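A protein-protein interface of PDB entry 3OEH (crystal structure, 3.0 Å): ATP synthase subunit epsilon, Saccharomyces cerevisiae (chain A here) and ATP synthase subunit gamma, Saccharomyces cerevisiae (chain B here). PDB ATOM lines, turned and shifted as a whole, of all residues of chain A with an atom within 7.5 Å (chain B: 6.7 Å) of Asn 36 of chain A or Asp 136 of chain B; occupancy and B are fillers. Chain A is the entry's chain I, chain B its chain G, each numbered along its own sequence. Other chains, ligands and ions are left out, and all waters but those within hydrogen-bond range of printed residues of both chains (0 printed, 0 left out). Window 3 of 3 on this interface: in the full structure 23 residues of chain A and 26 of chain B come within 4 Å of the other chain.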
ATOM      1  N   GLN A  30      39.046  -1.156 -25.506  1.00  0.00           N
ATOM      2  CA  GLN A  30      38.546  -2.518 -25.660  1.00  0.00           C
ATOM      3  C   GLN A  30      37.929  -2.959 -24.333  1.00  0.00           C
ATOM      4  O   GLN A  30      38.491  -3.793 -23.624  1.00  0.00           O
ATOM      5  CB  GLN A  30      39.695  -3.454 -26.061  1.00  0.00           C
ATOM      6  CG  GLN A  30      39.281  -4.837 -26.554  1.00  0.00           C
ATOM      7  CD  GLN A  30      40.444  -5.825 -26.590  1.00  0.00           C
ATOM      8  OE1 GLN A  30      41.600  -5.444 -26.789  1.00  0.00           O
ATOM      9  NE2 GLN A  30      40.137  -7.102 -26.396  1.00  0.00           N
ATOM     10  N   THR A  31      36.777  -2.378 -23.997  1.00  0.00           N
ATOM     11  CA  THR A  31      36.029  -2.733 -22.783  1.00  0.00           C
ATOM     12  C   THR A  31      35.563  -4.198 -22.793  1.00  0.00           C
ATOM     13  O   THR A  31      35.719  -4.902 -23.794  1.00  0.00           O
ATOM     14  CB  THR A  31      34.822  -1.774 -22.537  1.00  0.00           C
ATOM     15  OG1 THR A  31      34.376  -1.897 -21.181  1.00  0.00           O
ATOM     16  CG2 THR A  31      33.646  -2.079 -23.492  1.00  0.00           C
ATOM     17  N   ALA A  32      34.988  -4.647 -21.678  1.00  0.00           N
ATOM     18  CA  ALA A  32      34.578  -6.044 -21.516  1.00  0.00           C
ATOM     19  C   ALA A  32      33.676  -6.558 -22.642  1.00  0.00           C
ATOM     20  O   ALA A  32      33.921  -7.634 -23.186  1.00  0.00           O
ATOM     21  CB  ALA A  32      33.916  -6.255 -20.155  1.00  0.00           C
ATOM     22  N   SER A  33      32.654  -5.782 -22.995  1.00  0.00           N
ATOM     23  CA  SER A  33      31.673  -6.199 -24.005  1.00  0.00           C
ATOM     24  C   SER A  33      32.152  -6.100 -25.473  1.00  0.00           C
ATOM     25  O   SER A  33      31.401  -6.431 -26.392  1.00  0.00           O
ATOM     26  CB  SER A  33      30.347  -5.450 -23.812  1.00  0.00           C
ATOM     27  OG  SER A  33      30.432  -4.108 -24.263  1.00  0.00           O
ATOM     28  N   VAL A  34      33.385  -5.638 -25.685  1.00  0.00           N
ATOM     29  CA  VAL A  34      34.007  -5.641 -27.018  1.00  0.00           C
ATOM     30  C   VAL A  34      34.522  -7.048 -27.345  1.00  0.00           C
ATOM     31  O   VAL A  34      34.223  -7.598 -28.409  1.00  0.00           O
ATOM     32  CB  VAL A  34      35.148  -4.595 -27.123  1.00  0.00           C
ATOM     33  CG1 VAL A  34      35.808  -4.634 -28.498  1.00  0.00           C
ATOM     34  CG2 VAL A  34      34.617  -3.199 -26.833  1.00  0.00           C
ATOM     35  N   LEU A  35      35.284  -7.624 -26.412  1.00  0.00           N
ATOM     36  CA  LEU A  35      35.711  -9.029 -26.483  1.00  0.00           C
ATOM     37  C   LEU A  35      34.591 -10.014 -26.093  1.00  0.00           C
ATOM     38  O   LEU A  35      34.858 -11.183 -25.795  1.00  0.00           O
ATOM     39  CB  LEU A  35      36.966  -9.274 -25.629  1.00  0.00           C
ATOM     40  CG  LEU A  35      36.910  -9.061 -24.109  1.00  0.00           C
ATOM     41  CD1 LEU A  35      37.828 -10.042 -23.371  1.00  0.00           C
ATOM     42  CD2 LEU A  35      37.253  -7.622 -23.738  1.00  0.00           C
ATOM     43  N   ASN A  36      33.350  -9.525 -26.084  1.00  0.00           N
ATOM     44  CA  ASN A  36      32.166 -10.360 -25.874  1.00  0.00           C
ATOM     45  C   ASN A  36      31.176 -10.180 -27.024  1.00  0.00           C
ATOM     46  O   ASN A  36      30.265 -10.996 -27.218  1.00  0.00           O
ATOM     47  CB  ASN A  36      31.519 -10.082 -24.510  1.00  0.00           C
ATOM     48  CG  ASN A  36      32.075 -10.984 -23.389  1.00  0.00           C
ATOM     49  OD1 ASN A  36      33.290 -11.068 -23.166  1.00  0.00           O
ATOM     50  ND2 ASN A  36      31.173 -11.650 -22.674  1.00  0.00           N
ATOM     51  N   ARG A  37      31.373  -9.094 -27.772  1.00  0.00           N
ATOM     52  CA  ARG A  37      30.801  -8.915 -29.106  1.00  0.00           C
ATOM     53  C   ARG A  37      31.497  -9.882 -30.060  1.00  0.00           C
ATOM     54  O   ARG A  37      30.952 -10.251 -31.109  1.00  0.00           O
ATOM     55  CB  ARG A  37      31.020  -7.474 -29.586  1.00  0.00           C
ATOM     56  CG  ARG A  37      31.284  -7.317 -31.100  1.00  0.00           C
ATOM     57  CD  ARG A  37      31.729  -5.915 -31.496  1.00  0.00           C
ATOM     58  NE  ARG A  37      30.931  -4.891 -30.828  1.00  0.00           N
ATOM     59  CZ  ARG A  37      31.415  -3.994 -29.973  1.00  0.00           C
ATOM     60  NH1 ARG A  37      32.712  -3.957 -29.690  1.00  0.00           N
ATOM     61  NH2 ARG A  37      30.598  -3.115 -29.408  1.00  0.00           N
ATOM     62  N   SER A  38      32.704 -10.290 -29.679  1.00  0.00           N
ATOM     63  CA  SER A  38      33.573 -11.072 -30.545  1.00  0.00           C
ATOM     64  C   SER A  38      33.406 -12.588 -30.380  1.00  0.00           C
ATOM     65  O   SER A  38      33.710 -13.353 -31.299  1.00  0.00           O
ATOM     66  CB  SER A  38      35.026 -10.643 -30.326  1.00  0.00           C
ATOM     67  OG  SER A  38      35.204  -9.279 -30.690  1.00  0.00           O
ATOM     68  N   GLN A  39      32.906 -13.013 -29.221  1.00  0.00           N
ATOM     69  CA  GLN A  39      32.790 -14.439 -28.904  1.00  0.00           C
ATOM     70  C   GLN A  39      31.375 -14.973 -29.111  1.00  0.00           C
ATOM     71  O   GLN A  39      30.395 -14.329 -28.732  1.00  0.00           O
ATOM     72  CB  GLN A  39      33.262 -14.711 -27.467  1.00  0.00           C
ATOM     73  N   THR A  40      31.277 -16.156 -29.710  1.00  0.00           N
ATOM     74  CA  THR A  40      29.983 -16.795 -29.936  1.00  0.00           C
ATOM     75  C   THR A  40      29.980 -18.265 -29.512  1.00  0.00           C
ATOM     76  O   THR A  40      30.750 -19.078 -30.034  1.00  0.00           O
ATOM     77  CB  THR A  40      29.521 -16.677 -31.410  1.00  0.00           C
ATOM     78  N   ASP A  41      29.114 -18.586 -28.553  1.00  0.00           N
ATOM     79  CA  ASP A  41      28.845 -19.970 -28.167  1.00  0.00           C
ATOM     80  C   ASP A  41      27.665 -20.493 -28.987  1.00  0.00           C
ATOM     81  O   ASP A  41      26.684 -20.983 -28.433  1.00  0.00           O
ATOM     82  CB  ASP A  41      28.533 -20.062 -26.665  1.00  0.00           C
ATOM     83  CG  ASP A  41      29.657 -19.529 -25.792  1.00  0.00           C
ATOM     84  OD1 ASP A  41      30.829 -19.564 -26.226  1.00  0.00           O
ATOM     85  OD2 ASP A  41      29.366 -19.083 -24.660  1.00  0.00           O
ATOM     86  N   ARG B  30      21.648  -7.827 -15.276  1.00  0.00           N
ATOM     87  CA  ARG B  30      21.554  -8.329 -16.638  1.00  0.00           C
ATOM     88  C   ARG B  30      20.421  -7.650 -17.413  1.00  0.00           C
ATOM     89  O   ARG B  30      20.345  -7.766 -18.640  1.00  0.00           O
ATOM     90  CB  ARG B  30      21.366  -9.851 -16.615  1.00  0.00           C
ATOM     91  CG  ARG B  30      21.757 -10.563 -17.910  1.00  0.00           C
ATOM     92  CD  ARG B  30      21.986 -12.043 -17.675  1.00  0.00           C
ATOM     93  NE  ARG B  30      23.125 -12.271 -16.788  1.00  0.00           N
ATOM     94  CZ  ARG B  30      23.414 -13.433 -16.210  1.00  0.00           C
ATOM     95  NH1 ARG B  30      22.649 -14.502 -16.415  1.00  0.00           N
ATOM     96  NH2 ARG B  30      24.475 -13.530 -15.419  1.00  0.00           N
ATOM     97  N   LYS B  81      17.500 -21.359 -22.476  1.00  0.00           N
ATOM     98  CA  LYS B  81      17.186 -21.432 -21.048  1.00  0.00           C
ATOM     99  C   LYS B  81      15.691 -21.536 -20.775  1.00  0.00           C
ATOM    100  O   LYS B  81      14.867 -21.078 -21.567  1.00  0.00           O
ATOM    101  CB  LYS B  81      17.712 -20.194 -20.321  1.00  0.00           C
ATOM    102  CG  LYS B  81      19.214 -20.085 -20.182  1.00  0.00           C
ATOM    103  CD  LYS B  81      19.595 -18.620 -19.981  1.00  0.00           C
ATOM    104  CE  LYS B  81      20.808 -18.458 -19.090  1.00  0.00           C
ATOM    105  NZ  LYS B  81      20.469 -18.748 -17.665  1.00  0.00           N
ATOM    106  N   ILE B 133      22.178 -19.844 -26.913  1.00  0.00           N
ATOM    107  CA  ILE B 133      21.696 -18.582 -27.444  1.00  0.00           C
ATOM    108  C   ILE B 133      21.365 -17.453 -26.473  1.00  0.00           C
ATOM    109  O   ILE B 133      21.475 -16.282 -26.848  1.00  0.00           O
ATOM    110  CB  ILE B 133      20.573 -18.827 -28.491  1.00  0.00           C
ATOM    111  CG1 ILE B 133      21.176 -18.763 -29.898  1.00  0.00           C
ATOM    112  CG2 ILE B 133      19.384 -17.859 -28.333  1.00  0.00           C
ATOM    113  CD1 ILE B 133      22.303 -17.725 -30.067  1.00  0.00           C
ATOM    114  N   GLY B 134      20.979 -17.780 -25.243  1.00  0.00           N
ATOM    115  CA  GLY B 134      20.534 -16.747 -24.305  1.00  0.00           C
ATOM    116  C   GLY B 134      21.337 -16.637 -23.027  1.00  0.00           C
ATOM    117  O   GLY B 134      20.766 -16.663 -21.932  1.00  0.00           O
ATOM    118  N   LYS B 135      22.656 -16.502 -23.155  1.00  0.00           N
ATOM    119  CA  LYS B 135      23.544 -16.436 -21.982  1.00  0.00           C
ATOM    120  C   LYS B 135      23.955 -14.983 -21.723  1.00  0.00           C
ATOM    121  O   LYS B 135      23.570 -14.373 -20.714  1.00  0.00           O
ATOM    122  CB  LYS B 135      24.775 -17.328 -22.192  1.00  0.00           C
ATOM    123  CG  LYS B 135      25.167 -18.159 -20.973  1.00  0.00           C
ATOM    124  CD  LYS B 135      26.591 -18.704 -21.085  1.00  0.00           C
ATOM    125  CE  LYS B 135      27.616 -17.678 -20.598  1.00  0.00           C
ATOM    126  NZ  LYS B 135      29.017 -18.096 -20.875  1.00  0.00           N
ATOM    127  N   ASP B 136      24.753 -14.449 -22.646  1.00  0.00           N
ATOM    128  CA  ASP B 136      24.972 -13.017 -22.767  1.00  0.00           C
ATOM    129  C   ASP B 136      23.885 -12.453 -23.671  1.00  0.00           C
ATOM    130  O   ASP B 136      23.002 -13.184 -24.132  1.00  0.00           O
ATOM    131  CB  ASP B 136      26.350 -12.726 -23.375  1.00  0.00           C
ATOM    132  CG  ASP B 136      27.433 -12.510 -22.323  1.00  0.00           C
ATOM    133  OD1 ASP B 136      27.474 -13.262 -21.319  1.00  0.00           O
ATOM    134  OD2 ASP B 136      28.256 -11.584 -22.510  1.00  0.00           O
ATOM    135  N   ALA B 137      23.967 -11.149 -23.920  1.00  0.00           N
ATOM    136  CA  ALA B 137      23.076 -10.450 -24.836  1.00  0.00           C
ATOM    137  C   ALA B 137      23.320 -10.930 -26.265  1.00  0.00           C
ATOM    138  O   ALA B 137      24.334 -11.585 -26.530  1.00  0.00           O
ATOM    139  CB  ALA B 137      23.297  -8.946 -24.724  1.00  0.00           C
ATOM    140  N   PRO B 138      22.390 -10.623 -27.193  1.00  0.00           N
ATOM    141  CA  PRO B 138      22.690 -11.029 -28.554  1.00  0.00           C
ATOM    142  C   PRO B 138      23.542  -9.977 -29.254  1.00  0.00           C
ATOM    143  O   PRO B 138      23.466  -8.786 -28.933  1.00  0.00           O
ATOM    144  CB  PRO B 138      21.309 -11.145 -29.194  1.00  0.00           C
ATOM    145  CG  PRO B 138      20.440 -10.214 -28.412  1.00  0.00           C
ATOM    146  CD  PRO B 138      21.105  -9.904 -27.104  1.00  0.00           C
ATOM    147  N   THR B 139      24.359 -10.432 -30.194  1.00  0.00           N
ATOM    148  CA  THR B 139      25.253  -9.553 -30.928  1.00  0.00           C
ATOM    149  C   THR B 139      25.114  -9.729 -32.441  1.00  0.00           C
ATOM    150  O   THR B 139      24.780 -10.816 -32.928  1.00  0.00           O
ATOM    151  CB  THR B 139      26.701  -9.828 -30.553  1.00  0.00           C
ATOM    152  OG1 THR B 139      27.014 -11.190 -30.861  1.00  0.00           O
ATOM    153  CG2 THR B 139      26.916  -9.592 -29.070  1.00  0.00           C
ATOM    154  N   GLU B 142      26.506 -12.972 -33.835  1.00  0.00           N
ATOM    155  CA  GLU B 142      25.612 -14.127 -33.788  1.00  0.00           C
ATOM    156  C   GLU B 142      24.503 -13.879 -34.816  1.00  0.00           C
ATOM    157  O   GLU B 142      24.221 -14.730 -35.662  1.00  0.00           O
ATOM    158  CB  GLU B 142      25.055 -14.365 -32.375  1.00  0.00           C
ATOM    159  CG  GLU B 142      26.099 -14.177 -31.266  1.00  0.00           C
ATOM    160  CD  GLU B 142      25.991 -15.171 -30.102  1.00  0.00           C
ATOM    161  OE1 GLU B 142      24.868 -15.608 -29.766  1.00  0.00           O
ATOM    162  OE2 GLU B 142      27.044 -15.504 -29.511  1.00  0.00           O
ATOM    163  N   TYR B 226      15.119 -11.273 -26.042  1.00  0.00           N
ATOM    164  CA  TYR B 226      16.076 -11.483 -24.963  1.00  0.00           C
ATOM    165  C   TYR B 226      15.792 -10.608 -23.746  1.00  0.00           C
ATOM    166  O   TYR B 226      15.889 -11.077 -22.613  1.00  0.00           O
ATOM    167  CB  TYR B 226      17.504 -11.255 -25.469  1.00  0.00           C
ATOM    168  CG  TYR B 226      18.584 -11.299 -24.406  1.00  0.00           C
ATOM    169  CD1 TYR B 226      19.015 -12.513 -23.877  1.00  0.00           C
ATOM    170  CD2 TYR B 226      19.187 -10.127 -23.949  1.00  0.00           C
ATOM    171  CE1 TYR B 226      20.005 -12.558 -22.913  1.00  0.00           C
ATOM    172  CE2 TYR B 226      20.179 -10.162 -22.991  1.00  0.00           C
ATOM    173  CZ  TYR B 226      20.585 -11.382 -22.476  1.00  0.00           C
ATOM    174  OH  TYR B 226      21.575 -11.434 -21.514  1.00  0.00           O
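The side-chain amino group (NZ) of Lys 135 of chain B lies within salt-bridge range of the side-chain carboxylate (OD2) of Asp 41 of chain A.
The side-chain carboxylate of Asp 136 of chain B sits at hydrogen-bond distance from the side-chain amide nitrogen of Asn 36 of chain A, 2.9 Å away.
Among the printed residues, 6 pairs touch across the chains.
Among the printed residues, Asp or Glu carboxylates within 4 Å of a Lys or Arg side-chain nitrogen of the other chain: Asp 41 of chain A with Lys 135 of chain B.
Asn 36 of chain A touches just one residue of chain B: Asp 136 (2.9 Å).
Asp 136 of chain B touches just one residue of chain A: Asn 36 (2.9 Å).
Of the printed residues of chain B, Arg 37 of chain A touches Thr 139 (3.9 Å).
Printed residues of chain B within 4 Å of Gln 39 of chain A: Glu 142.
Printed residues of chain B within 4 Å of Thr 40 of chain A: Glu 142.
Printed residues of chain A within 4 Å of Thr 139 of chain B: Arg 37.
Lys 81 of chain B touches none of the printed residues of chain A.
Ile 133 of chain B touches none of the printed residues of chain A.
Arg 37 of chain A touches Thr 139 of chain B (CA to CG2, 3.9 Å).
OE2 of Glu 142 of chain B touches O of Gln 39 of chain A (3.6 Å).
Thr 40 of chain A touches Glu 142 of chain B (CA to OE2, 3.2 Å).
Glu 142 of chain B touches Asp 41 of chain A (OE2 to N, 3.8 Å).
The backbone carbonyl oxygen (O) of Asp 136 of chain B sits close to the side-chain hydroxyl (OH) of Tyr 226 of chain B.
O of Ala 32 of chain A sits close to OD1 of Asn 36 of chain A, 3.5 Å away.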
